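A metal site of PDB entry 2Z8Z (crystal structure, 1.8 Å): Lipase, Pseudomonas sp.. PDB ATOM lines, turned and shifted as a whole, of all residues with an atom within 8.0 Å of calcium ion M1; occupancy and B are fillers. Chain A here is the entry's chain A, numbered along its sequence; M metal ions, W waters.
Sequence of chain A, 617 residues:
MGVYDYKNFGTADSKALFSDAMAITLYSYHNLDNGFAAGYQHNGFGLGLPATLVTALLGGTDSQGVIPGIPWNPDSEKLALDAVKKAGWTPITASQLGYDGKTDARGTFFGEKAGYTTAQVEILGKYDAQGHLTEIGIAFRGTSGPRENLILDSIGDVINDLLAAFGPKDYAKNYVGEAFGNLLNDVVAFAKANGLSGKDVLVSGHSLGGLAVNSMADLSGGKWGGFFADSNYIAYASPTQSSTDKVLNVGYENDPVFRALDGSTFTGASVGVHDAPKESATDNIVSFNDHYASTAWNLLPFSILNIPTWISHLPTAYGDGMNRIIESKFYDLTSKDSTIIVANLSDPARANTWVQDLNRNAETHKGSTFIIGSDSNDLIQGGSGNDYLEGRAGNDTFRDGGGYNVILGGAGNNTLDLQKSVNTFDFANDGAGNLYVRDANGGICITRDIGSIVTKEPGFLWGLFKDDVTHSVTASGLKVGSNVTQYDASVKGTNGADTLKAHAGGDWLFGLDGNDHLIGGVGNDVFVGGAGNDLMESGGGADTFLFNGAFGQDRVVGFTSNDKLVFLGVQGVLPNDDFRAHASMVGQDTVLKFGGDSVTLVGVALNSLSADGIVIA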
ATOM      1  N   VAL A 522     -22.021  -5.424  12.953  1.00  0.00           N
ATOM      2  CA  VAL A 522     -20.952  -6.400  13.159  1.00  0.00           C
ATOM      3  C   VAL A 522     -21.094  -7.080  14.477  1.00  0.00           C
ATOM      4  O   VAL A 522     -20.392  -8.020  14.748  1.00  0.00           O
ATOM      5  CB  VAL A 522     -19.571  -5.688  13.153  1.00  0.00           C
ATOM      6  CG1 VAL A 522     -19.325  -4.942  11.856  1.00  0.00           C
ATOM      7  CG2 VAL A 522     -19.511  -4.745  14.339  1.00  0.00           C
ATOM      8  N   GLY A 523     -21.994  -6.597  15.354  1.00  0.00           N
ATOM      9  CA  GLY A 523     -22.267  -7.263  16.604  1.00  0.00           C
ATOM     10  C   GLY A 523     -23.276  -8.413  16.486  1.00  0.00           C
ATOM     11  O   GLY A 523     -23.779  -8.682  15.428  1.00  0.00           O
ATOM     12  N   ASN A 524     -23.528  -9.025  17.634  1.00  0.00           N
ATOM     13  CA  ASN A 524     -24.416 -10.157  17.820  1.00  0.00           C
ATOM     14  C   ASN A 524     -25.851  -9.614  18.015  1.00  0.00           C
ATOM     15  O   ASN A 524     -26.238  -9.118  19.069  1.00  0.00           O
ATOM     16  CB  ASN A 524     -23.971 -11.010  18.991  1.00  0.00           C
ATOM     17  CG  ASN A 524     -22.550 -11.542  18.856  1.00  0.00           C
ATOM     18  OD1 ASN A 524     -21.952 -11.524  17.794  1.00  0.00           O
ATOM     19  ND2 ASN A 524     -22.042 -12.070  19.955  1.00  0.00           N
ATOM     20  N   SER A 538     -27.559  -9.896   8.279  1.00  0.00           N
ATOM     21  CA  SER A 538     -26.751 -10.166   9.457  1.00  0.00           C
ATOM     22  C   SER A 538     -25.799  -9.009   9.833  1.00  0.00           C
ATOM     23  O   SER A 538     -25.693  -8.577  11.019  1.00  0.00           O
ATOM     24  CB  SER A 538     -25.826 -11.399   9.176  1.00  0.00           C
ATOM     25  OG  SER A 538     -24.815 -11.477  10.177  1.00  0.00           O
ATOM     26  N   GLY A 539     -25.038  -8.602   8.842  1.00  0.00           N
ATOM     27  CA  GLY A 539     -23.996  -7.594   8.984  1.00  0.00           C
ATOM     28  C   GLY A 539     -22.709  -8.004   9.717  1.00  0.00           C
ATOM     29  O   GLY A 539     -21.781  -7.173   9.861  1.00  0.00           O
ATOM     30  N   GLY A 540     -22.636  -9.269  10.083  1.00  0.00           N
ATOM     31  CA  GLY A 540     -21.484  -9.895  10.749  1.00  0.00           C
ATOM     32  C   GLY A 540     -21.832 -10.340  12.161  1.00  0.00           C
ATOM     33  O   GLY A 540     -22.959 -10.165  12.640  1.00  0.00           O
ATOM     34  N   GLY A 541     -20.895 -10.960  12.878  1.00  0.00           N
ATOM     35  CA  GLY A 541     -21.163 -11.436  14.214  1.00  0.00           C
ATOM     36  C   GLY A 541     -21.889 -12.786  14.234  1.00  0.00           C
ATOM     37  O   GLY A 541     -22.025 -13.463  13.203  1.00  0.00           O
ATOM     38  N   ALA A 542     -22.282 -13.159  15.431  1.00  0.00           N
ATOM     39  CA  ALA A 542     -23.012 -14.407  15.709  1.00  0.00           C
ATOM     40  C   ALA A 542     -24.430 -13.954  16.015  1.00  0.00           C
ATOM     41  O   ALA A 542     -24.769 -13.517  17.128  1.00  0.00           O
ATOM     42  CB  ALA A 542     -22.356 -15.156  16.873  1.00  0.00           C
ATOM     43  N   ASP A 543     -25.271 -14.089  14.983  1.00  0.00           N
ATOM     44  CA  ASP A 543     -26.610 -13.560  14.993  1.00  0.00           C
ATOM     45  C   ASP A 543     -27.625 -14.701  15.168  1.00  0.00           C
ATOM     46  O   ASP A 543     -27.391 -15.799  14.784  1.00  0.00           O
ATOM     47  CB  ASP A 543     -26.893 -12.826  13.699  1.00  0.00           C
ATOM     48  CG  ASP A 543     -26.084 -11.512  13.553  1.00  0.00           C
ATOM     49  OD1 ASP A 543     -25.735 -10.913  14.576  1.00  0.00           O
ATOM     50  OD2 ASP A 543     -25.967 -11.020  12.416  1.00  0.00           O
ATOM     51  N   THR A 544     -28.775 -14.339  15.701  1.00  0.00           N
ATOM     52  CA  THR A 544     -29.907 -15.216  15.901  1.00  0.00           C
ATOM     53  C   THR A 544     -31.123 -14.629  15.151  1.00  0.00           C
ATOM     54  O   THR A 544     -31.387 -13.438  15.276  1.00  0.00           O
ATOM     55  CB  THR A 544     -30.261 -15.260  17.392  1.00  0.00           C
ATOM     56  OG1 THR A 544     -29.142 -15.716  18.135  1.00  0.00           O
ATOM     57  CG2 THR A 544     -31.456 -16.141  17.650  1.00  0.00           C
ATOM     58  N   PHE A 545     -31.843 -15.461  14.393  1.00  0.00           N
ATOM     59  CA  PHE A 545     -33.052 -15.031  13.656  1.00  0.00           C
ATOM     60  C   PHE A 545     -34.207 -15.855  14.194  1.00  0.00           C
ATOM     61  O   PHE A 545     -34.150 -17.087  14.170  1.00  0.00           O
ATOM     62  CB  PHE A 545     -32.895 -15.288  12.184  1.00  0.00           C
ATOM     63  CG  PHE A 545     -31.739 -14.547  11.560  1.00  0.00           C
ATOM     64  CD1 PHE A 545     -31.933 -13.380  10.868  1.00  0.00           C
ATOM     65  CD2 PHE A 545     -30.440 -15.029  11.684  1.00  0.00           C
ATOM     66  CE1 PHE A 545     -30.837 -12.685  10.274  1.00  0.00           C
ATOM     67  CE2 PHE A 545     -29.338 -14.322  11.125  1.00  0.00           C
ATOM     68  CZ  PHE A 545     -29.543 -13.170  10.406  1.00  0.00           C
ATOM     69  N   GLY A 558     -26.595 -12.922   4.511  1.00  0.00           N
ATOM     70  CA  GLY A 558     -25.325 -12.968   5.276  1.00  0.00           C
ATOM     71  C   GLY A 558     -25.270 -14.011   6.337  1.00  0.00           C
ATOM     72  O   GLY A 558     -24.475 -13.905   7.275  1.00  0.00           O
ATOM     73  N   PHE A 559     -26.100 -15.043   6.223  1.00  0.00           N
ATOM     74  CA  PHE A 559     -26.102 -16.134   7.213  1.00  0.00           C
ATOM     75  C   PHE A 559     -24.820 -16.971   7.097  1.00  0.00           C
ATOM     76  O   PHE A 559     -24.511 -17.425   5.996  1.00  0.00           O
ATOM     77  CB  PHE A 559     -27.323 -17.094   6.975  1.00  0.00           C
ATOM     78  CG  PHE A 559     -27.513 -18.145   8.049  1.00  0.00           C
ATOM     79  CD1 PHE A 559     -28.242 -17.855   9.223  1.00  0.00           C
ATOM     80  CD2 PHE A 559     -27.093 -19.442   7.867  1.00  0.00           C
ATOM     81  CE1 PHE A 559     -28.445 -18.804  10.206  1.00  0.00           C
ATOM     82  CE2 PHE A 559     -27.293 -20.424   8.864  1.00  0.00           C
ATOM     83  CZ  PHE A 559     -27.993 -20.117  10.012  1.00  0.00           C
ATOM     84  N   THR A 560     -24.159 -17.180   8.218  1.00  0.00           N
ATOM     85  CA  THR A 560     -22.950 -18.013   8.297  1.00  0.00           C
ATOM     86  C   THR A 560     -23.101 -19.066   9.358  1.00  0.00           C
ATOM     87  O   THR A 560     -24.095 -19.059  10.133  1.00  0.00           O
ATOM     88  CB  THR A 560     -21.678 -17.187   8.549  1.00  0.00           C
ATOM     89  OG1 THR A 560     -21.640 -16.782   9.908  1.00  0.00           O
ATOM     90  CG2 THR A 560     -21.596 -16.010   7.597  1.00  0.00           C
ATOM     91  N   SER A 561     -22.098 -19.954   9.430  1.00  0.00           N
ATOM     92  CA  SER A 561     -22.108 -21.123  10.344  1.00  0.00           C
ATOM     93  C   SER A 561     -22.341 -20.759  11.812  1.00  0.00           C
ATOM     94  O   SER A 561     -22.859 -21.564  12.561  1.00  0.00           O
ATOM     95  CB  SER A 561     -20.746 -21.862  10.259  1.00  0.00           C
ATOM     96  OG  SER A 561     -20.742 -22.435   9.008  1.00  0.00           O
ATOM     97  N   ASN A 562     -21.856 -19.596  12.239  1.00  0.00           N
ATOM     98  CA  ASN A 562     -21.989 -19.195  13.636  1.00  0.00           C
ATOM     99  C   ASN A 562     -23.301 -18.475  14.014  1.00  0.00           C
ATOM    100  O   ASN A 562     -23.516 -18.055  15.187  1.00  0.00           O
ATOM    101  CB  ASN A 562     -20.749 -18.379  14.093  1.00  0.00           C
ATOM    102  CG  ASN A 562     -20.779 -16.927  13.657  1.00  0.00           C
ATOM    103  OD1 ASN A 562     -21.492 -16.545  12.729  1.00  0.00           O
ATOM    104  ND2 ASN A 562     -19.893 -16.129  14.242  1.00  0.00           N
ATOM    105  N   ASP A 563     -24.178 -18.358  13.016  1.00  0.00           N
ATOM    106  CA  ASP A 563     -25.505 -17.812  13.181  1.00  0.00           C
ATOM    107  C   ASP A 563     -26.535 -18.922  13.423  1.00  0.00           C
ATOM    108  O   ASP A 563     -26.241 -20.114  13.215  1.00  0.00           O
ATOM    109  CB  ASP A 563     -25.882 -17.021  11.964  1.00  0.00           C
ATOM    110  CG  ASP A 563     -24.860 -15.923  11.674  1.00  0.00           C
ATOM    111  OD1 ASP A 563     -24.419 -15.315  12.634  1.00  0.00           O
ATOM    112  OD2 ASP A 563     -24.486 -15.769  10.522  1.00  0.00           O
ATOM    113  N   LYS A 564     -27.702 -18.520  13.937  1.00  0.00           N
ATOM    114  CA  LYS A 564     -28.731 -19.489  14.279  1.00  0.00           C
ATOM    115  C   LYS A 564     -30.107 -19.003  13.851  1.00  0.00           C
ATOM    116  O   LYS A 564     -30.465 -17.820  14.024  1.00  0.00           O
ATOM    117  CB  LYS A 564     -28.700 -19.772  15.780  1.00  0.00           C
ATOM    118  CG  LYS A 564     -29.593 -20.927  16.246  1.00  0.00           C
ATOM    119  CD  LYS A 564     -29.291 -21.332  17.695  1.00  0.00           C
ATOM    120  CE  LYS A 564     -29.591 -20.215  18.681  1.00  0.00           C
ATOM    121  NZ  LYS A 564     -29.268 -20.552  20.135  1.00  0.00           N
HETATM  122 CA    CA M   1     -22.334 -14.880  11.394  1.00  0.00          CA
HETATM  123 CA    CA M   2     -24.839  -8.960  13.248  1.00  0.00          CA
HETATM  124  O   HOH W   1     -22.825 -13.178   9.974  1.00  0.00           O
HETATM  125  O   HOH W   2     -20.020 -14.190  11.115  1.00  0.00           O
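Water W1 lies within hydrogen-bond range of OG of Ser 538 (2.6 Å) and O of Gly 558 (3.2 Å).
Within 4 Å of calcium ion M1: Gly 541, Thr 560, Asn 562 and Asp 563.
Along chain A the residues within 4 Å of calcium ion M1 span positions 541 to 563.
Calcium ion M1 is bound by water W1 (2.3 Å), the side-chain amide oxygen (OD1) of Asn 562 (2.3 Å), the backbone carbonyl oxygen (O) of Gly 541 (2.3 Å), water W2 (2.4 Å), the side-chain carboxylate (OD1) of Asp 563 (2.5 Å), the side-chain carboxylate (OD2) of Asp 563 (2.5 Å) and the side-chain hydroxyl (OG1) of Thr 560 (2.5 Å).
Calcium ion M1 has seven donor atoms within binding distance.
The backbone NH of Asp 543 sits close to the side-chain carboxylate of Asp 563, 2.8 Å away.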
